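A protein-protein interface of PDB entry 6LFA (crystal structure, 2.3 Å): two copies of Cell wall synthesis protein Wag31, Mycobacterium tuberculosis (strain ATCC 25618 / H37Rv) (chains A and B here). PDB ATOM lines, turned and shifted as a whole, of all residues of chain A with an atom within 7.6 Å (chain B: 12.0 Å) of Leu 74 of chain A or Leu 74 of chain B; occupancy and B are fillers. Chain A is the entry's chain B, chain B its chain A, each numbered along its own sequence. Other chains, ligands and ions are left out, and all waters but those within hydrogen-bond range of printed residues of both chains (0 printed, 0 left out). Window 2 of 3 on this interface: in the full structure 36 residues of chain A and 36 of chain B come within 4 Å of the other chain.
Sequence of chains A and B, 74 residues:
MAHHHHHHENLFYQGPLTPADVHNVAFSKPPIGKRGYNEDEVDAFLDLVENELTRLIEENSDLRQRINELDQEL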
ATOM      1  N   ASN A  68     -16.037 -17.286  11.181  1.00  0.00           N
ATOM      2  CA  ASN A  68     -15.165 -16.246  11.706  1.00  0.00           C
ATOM      3  C   ASN A  68     -15.797 -14.870  11.506  1.00  0.00           C
ATOM      4  O   ASN A  68     -15.894 -14.064  12.442  1.00  0.00           O
ATOM      5  CB  ASN A  68     -13.819 -16.377  11.003  1.00  0.00           C
ATOM      6  CG  ASN A  68     -12.886 -15.243  11.276  1.00  0.00           C
ATOM      7  OD1 ASN A  68     -13.215 -14.069  11.092  1.00  0.00           O
ATOM      8  ND2 ASN A  68     -11.676 -15.592  11.670  1.00  0.00           N
ATOM      9  N   GLU A  69     -16.268 -14.601  10.289  1.00  0.00           N
ATOM     10  CA  GLU A  69     -16.889 -13.315  10.019  1.00  0.00           C
ATOM     11  C   GLU A  69     -18.082 -13.094  10.931  1.00  0.00           C
ATOM     12  O   GLU A  69     -18.318 -11.969  11.391  1.00  0.00           O
ATOM     13  CB  GLU A  69     -17.305 -13.224   8.552  1.00  0.00           C
ATOM     14  CG  GLU A  69     -16.159 -13.444   7.542  1.00  0.00           C
ATOM     15  CD  GLU A  69     -16.674 -13.778   6.128  1.00  0.00           C
ATOM     16  OE1 GLU A  69     -17.886 -14.100   5.979  1.00  0.00           O
ATOM     17  OE2 GLU A  69     -15.869 -13.724   5.164  1.00  0.00           O
ATOM     18  N   LEU A  70     -18.828 -14.164  11.236  1.00  0.00           N
ATOM     19  CA  LEU A  70     -20.035 -13.981  12.028  1.00  0.00           C
ATOM     20  C   LEU A  70     -19.684 -13.753  13.491  1.00  0.00           C
ATOM     21  O   LEU A  70     -20.325 -12.944  14.175  1.00  0.00           O
ATOM     22  CB  LEU A  70     -20.971 -15.178  11.858  1.00  0.00           C
ATOM     23  CG  LEU A  70     -21.559 -15.330  10.455  1.00  0.00           C
ATOM     24  CD1 LEU A  70     -22.400 -16.634  10.340  1.00  0.00           C
ATOM     25  CD2 LEU A  70     -22.380 -14.113  10.095  1.00  0.00           C
ATOM     26  N   ASP A  71     -18.647 -14.426  13.979  1.00  0.00           N
ATOM     27  CA  ASP A  71     -18.238 -14.209  15.360  1.00  0.00           C
ATOM     28  C   ASP A  71     -17.735 -12.791  15.553  1.00  0.00           C
ATOM     29  O   ASP A  71     -18.001 -12.166  16.586  1.00  0.00           O
ATOM     30  CB  ASP A  71     -17.152 -15.204  15.768  1.00  0.00           C
ATOM     31  CG  ASP A  71     -17.653 -16.619  15.824  1.00  0.00           C
ATOM     32  OD1 ASP A  71     -17.078 -17.444  15.096  1.00  0.00           O
ATOM     33  OD2 ASP A  71     -18.620 -16.915  16.565  1.00  0.00           O
ATOM     34  N   GLN A  72     -17.002 -12.271  14.568  1.00  0.00           N
ATOM     35  CA  GLN A  72     -16.540 -10.892  14.643  1.00  0.00           C
ATOM     36  C   GLN A  72     -17.685  -9.903  14.760  1.00  0.00           C
ATOM     37  O   GLN A  72     -17.487  -8.792  15.263  1.00  0.00           O
ATOM     38  CB  GLN A  72     -15.722 -10.554  13.420  1.00  0.00           C
ATOM     39  CG  GLN A  72     -14.309 -11.020  13.523  1.00  0.00           C
ATOM     40  CD  GLN A  72     -13.529 -10.652  12.295  1.00  0.00           C
ATOM     41  OE1 GLN A  72     -13.957 -10.929  11.168  1.00  0.00           O
ATOM     42  NE2 GLN A  72     -12.382 -10.003  12.498  1.00  0.00           N
ATOM     43  N   GLU A  73     -18.860 -10.272  14.280  1.00  0.00           N
ATOM     44  CA  GLU A  73     -20.043  -9.439  14.373  1.00  0.00           C
ATOM     45  C   GLU A  73     -20.834  -9.708  15.640  1.00  0.00           C
ATOM     46  O   GLU A  73     -21.877  -9.087  15.850  1.00  0.00           O
ATOM     47  CB  GLU A  73     -20.933  -9.664  13.150  1.00  0.00           C
ATOM     48  CG  GLU A  73     -20.308  -9.149  11.874  1.00  0.00           C
ATOM     49  CD  GLU A  73     -21.169  -9.385  10.640  1.00  0.00           C
ATOM     50  OE1 GLU A  73     -22.168 -10.149  10.724  1.00  0.00           O
ATOM     51  OE2 GLU A  73     -20.825  -8.808   9.578  1.00  0.00           O
ATOM     52  N   LEU A  74     -20.369 -10.619  16.484  1.00  0.00           N
ATOM     53  CA  LEU A  74     -21.067 -10.914  17.722  1.00  0.00           C
ATOM     54  C   LEU A  74     -20.458 -10.127  18.879  1.00  0.00           C
ATOM     55  O   LEU A  74     -21.188  -9.796  19.819  1.00  0.00           O
ATOM     56  CB  LEU A  74     -21.030 -12.416  18.010  1.00  0.00           C
ATOM     57  CG  LEU A  74     -22.403 -13.102  18.118  1.00  0.00           C
ATOM     58  CD1 LEU A  74     -23.303 -12.839  16.903  1.00  0.00           C
ATOM     59  CD2 LEU A  74     -22.210 -14.589  18.338  1.00  0.00           C
ATOM     60  OXT LEU A  74     -19.261  -9.786  18.882  1.00  0.00           O
ATOM     61  N   GLN B  65     -24.507 -26.321  10.963  1.00  0.00           N
ATOM     62  CA  GLN B  65     -25.338 -26.103  12.142  1.00  0.00           C
ATOM     63  C   GLN B  65     -24.881 -24.873  12.913  1.00  0.00           C
ATOM     64  O   GLN B  65     -25.709 -24.065  13.354  1.00  0.00           O
ATOM     65  CB  GLN B  65     -25.333 -27.343  13.023  1.00  0.00           C
ATOM     66  CG  GLN B  65     -26.200 -28.428  12.404  1.00  0.00           C
ATOM     67  CD  GLN B  65     -26.096 -29.768  13.107  1.00  0.00           C
ATOM     68  OE1 GLN B  65     -25.284 -30.622  12.728  1.00  0.00           O
ATOM     69  NE2 GLN B  65     -26.940 -29.973  14.123  1.00  0.00           N
ATOM     70  N   ARG B  66     -23.567 -24.694  13.060  1.00  0.00           N
ATOM     71  CA  ARG B  66     -23.092 -23.533  13.791  1.00  0.00           C
ATOM     72  C   ARG B  66     -23.430 -22.255  13.055  1.00  0.00           C
ATOM     73  O   ARG B  66     -23.732 -21.240  13.683  1.00  0.00           O
ATOM     74  CB  ARG B  66     -21.592 -23.629  14.025  1.00  0.00           C
ATOM     75  CG  ARG B  66     -21.224 -24.809  14.889  1.00  0.00           C
ATOM     76  CD  ARG B  66     -21.825 -24.749  16.305  1.00  0.00           C
ATOM     77  NE  ARG B  66     -21.479 -25.943  17.091  1.00  0.00           N
ATOM     78  CZ  ARG B  66     -22.257 -27.021  17.240  1.00  0.00           C
ATOM     79  NH1 ARG B  66     -23.458 -27.081  16.672  1.00  0.00           N
ATOM     80  NH2 ARG B  66     -21.830 -28.048  17.970  1.00  0.00           N
ATOM     81  N   ILE B  67     -23.407 -22.287  11.728  1.00  0.00           N
ATOM     82  CA  ILE B  67     -23.724 -21.077  11.003  1.00  0.00           C
ATOM     83  C   ILE B  67     -25.203 -20.764  11.145  1.00  0.00           C
ATOM     84  O   ILE B  67     -25.591 -19.596  11.230  1.00  0.00           O
ATOM     85  CB  ILE B  67     -23.278 -21.222   9.539  1.00  0.00           C
ATOM     86  CG1 ILE B  67     -21.777 -20.974   9.442  1.00  0.00           C
ATOM     87  CG2 ILE B  67     -24.052 -20.276   8.621  1.00  0.00           C
ATOM     88  CD1 ILE B  67     -21.136 -21.624   8.246  1.00  0.00           C
ATOM     89  N   ASN B  68     -26.050 -21.787  11.212  1.00  0.00           N
ATOM     90  CA  ASN B  68     -27.473 -21.524  11.420  1.00  0.00           C
ATOM     91  C   ASN B  68     -27.720 -20.936  12.802  1.00  0.00           C
ATOM     92  O   ASN B  68     -28.532 -20.015  12.957  1.00  0.00           O
ATOM     93  CB  ASN B  68     -28.283 -22.804  11.230  1.00  0.00           C
ATOM     94  CG  ASN B  68     -28.378 -23.214   9.771  1.00  0.00           C
ATOM     95  OD1 ASN B  68     -28.125 -22.406   8.867  1.00  0.00           O
ATOM     96  ND2 ASN B  68     -28.742 -24.468   9.529  1.00  0.00           N
ATOM     97  N   GLU B  69     -27.010 -21.441  13.816  1.00  0.00           N
ATOM     98  CA  GLU B  69     -27.191 -20.923  15.171  1.00  0.00           C
ATOM     99  C   GLU B  69     -26.706 -19.488  15.277  1.00  0.00           C
ATOM    100  O   GLU B  69     -27.384 -18.635  15.867  1.00  0.00           O
ATOM    101  CB  GLU B  69     -26.458 -21.807  16.184  1.00  0.00           C
ATOM    102  CG  GLU B  69     -27.053 -23.219  16.329  1.00  0.00           C
ATOM    103  CD  GLU B  69     -28.550 -23.211  16.645  1.00  0.00           C
ATOM    104  OE1 GLU B  69     -29.031 -22.234  17.269  1.00  0.00           O
ATOM    105  OE2 GLU B  69     -29.243 -24.182  16.255  1.00  0.00           O
ATOM    106  N   LEU B  70     -25.536 -19.198  14.709  1.00  0.00           N
ATOM    107  CA  LEU B  70     -25.099 -17.815  14.617  1.00  0.00           C
ATOM    108  C   LEU B  70     -26.136 -16.958  13.901  1.00  0.00           C
ATOM    109  O   LEU B  70     -26.542 -15.909  14.412  1.00  0.00           O
ATOM    110  CB  LEU B  70     -23.759 -17.742  13.901  1.00  0.00           C
ATOM    111  CG  LEU B  70     -22.605 -18.384  14.655  1.00  0.00           C
ATOM    112  CD1 LEU B  70     -21.276 -18.027  13.979  1.00  0.00           C
ATOM    113  CD2 LEU B  70     -22.615 -17.977  16.134  1.00  0.00           C
ATOM    114  N   ASP B  71     -26.576 -17.380  12.709  1.00  0.00           N
ATOM    115  CA  ASP B  71     -27.541 -16.583  11.958  1.00  0.00           C
ATOM    116  C   ASP B  71     -28.804 -16.352  12.766  1.00  0.00           C
ATOM    117  O   ASP B  71     -29.543 -15.402  12.488  1.00  0.00           O
ATOM    118  CB  ASP B  71     -27.895 -17.256  10.619  1.00  0.00           C
ATOM    119  CG  ASP B  71     -26.884 -16.938   9.500  1.00  0.00           C
ATOM    120  OD1 ASP B  71     -26.183 -15.888   9.564  1.00  0.00           O
ATOM    121  OD2 ASP B  71     -26.809 -17.742   8.538  1.00  0.00           O
ATOM    122  N   GLN B  72     -29.065 -17.219  13.747  1.00  0.00           N
ATOM    123  CA  GLN B  72     -30.164 -16.990  14.675  1.00  0.00           C
ATOM    124  C   GLN B  72     -29.814 -15.901  15.681  1.00  0.00           C
ATOM    125  O   GLN B  72     -30.634 -15.021  15.966  1.00  0.00           O
ATOM    126  CB  GLN B  72     -30.518 -18.301  15.384  1.00  0.00           C
ATOM    127  CG  GLN B  72     -31.677 -19.072  14.734  1.00  0.00           C
ATOM    128  CD  GLN B  72     -31.986 -20.402  15.435  1.00  0.00           C
ATOM    129  OE1 GLN B  72     -31.161 -20.938  16.183  1.00  0.00           O
ATOM    130  NE2 GLN B  72     -33.180 -20.936  15.188  1.00  0.00           N
ATOM    131  N   GLU B  73     -28.601 -15.954  16.237  1.00  0.00           N
ATOM    132  CA  GLU B  73     -28.150 -14.953  17.199  1.00  0.00           C
ATOM    133  C   GLU B  73     -28.000 -13.556  16.606  1.00  0.00           C
ATOM    134  O   GLU B  73     -27.912 -12.588  17.365  1.00  0.00           O
ATOM    135  CB  GLU B  73     -26.794 -15.341  17.769  1.00  0.00           C
ATOM    136  CG  GLU B  73     -26.794 -16.478  18.734  1.00  0.00           C
ATOM    137  CD  GLU B  73     -25.379 -16.795  19.173  1.00  0.00           C
ATOM    138  OE1 GLU B  73     -25.043 -16.577  20.360  1.00  0.00           O
ATOM    139  OE2 GLU B  73     -24.586 -17.219  18.303  1.00  0.00           O
ATOM    140  N   LEU B  74     -27.899 -13.427  15.289  1.00  0.00           N
ATOM    141  CA  LEU B  74     -27.655 -12.124  14.663  1.00  0.00           C
ATOM    142  C   LEU B  74     -28.957 -11.434  14.282  1.00  0.00           C
ATOM    143  O   LEU B  74     -28.957 -10.399  13.595  1.00  0.00           O
ATOM    144  CB  LEU B  74     -26.786 -12.273  13.411  1.00  0.00           C
ATOM    145  CG  LEU B  74     -25.276 -12.142  13.535  1.00  0.00           C
ATOM    146  CD1 LEU B  74     -24.704 -12.134  12.133  1.00  0.00           C
ATOM    147  CD2 LEU B  74     -24.868 -10.897  14.292  1.00  0.00           C
ATOM    148  OXT LEU B  74     -30.031 -11.915  14.642  1.00  0.00           O
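Among the printed residues, merely in contact across the chains: Glu 73 of chain A with Leu 74 of chain B (3.5 Å), Leu 74 of chain A with Glu 73 of chain B (3.5 Å), Leu 70 of chain A with Leu 70 of chain B (3.6 Å), Leu 74 of chain A with Leu 74 of chain B (3.6 Å), Leu 70 of chain A with Leu 74 of chain B (3.7 Å), Asp 71 of chain A with Leu 70 of chain B (3.9 Å) and Leu 70 of chain A with Asp 71 of chain B (3.9 Å).
Asn 68 of chain A touches none of the printed residues of chain B. Of the printed residues of chain B, Leu 70 of chain A touches Leu 70 (3.6 Å), Asp 71 (3.9 Å) and Leu 74 (3.7 Å). Of chain B, only Leu 70 (3.9 Å) comes within 4 Å of Asp 71 of chain A. Of chain B, only Glu 73 and Leu 74 come within 4 Å of Leu 74 of chain A. Of the printed residues of chain A, Leu 70 of chain B touches Leu 70 (3.6 Å) and Asp 71 (3.9 Å). Printed residues of chain A within 4 Å of Asp 71 of chain B: Leu 70. Of the printed residues of chain A, Glu 73 of chain B touches Leu 74. Of chain A, only Leu 70 (3.7 Å), Glu 73 (3.5 Å) and Leu 74 (3.6 Å) come within 4 Å of Leu 74 of chain B. The nearest residue of chain B that does not touch Leu 74 of chain A is Leu 70 of chain B (4.1 Å).
Hydrophobic or aromatic side chains of chain A that line the printed part of chain B: Leu 70 and Leu 74. Hydrophobic or aromatic side chains of chain B within 4 Å of the printed part of chain A: Leu 70 and Leu 74. Among the printed residues, 7 pairs touch across the chains.
Leu 70 of chain A touches its own counterpart, Leu 70 of chain B. Leu 70 of chain A touches Asp 71 of chain B, and with the chains exchanged Asp 71 of chain A touches Leu 70 of chain B. Glu 73 of chain A touches Leu 74 of chain B, and with the chains exchanged Leu 74 of chain A touches Glu 73 of chain B. Leu 74 of chain B touches its own counterpart, Leu 74 of chain A.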
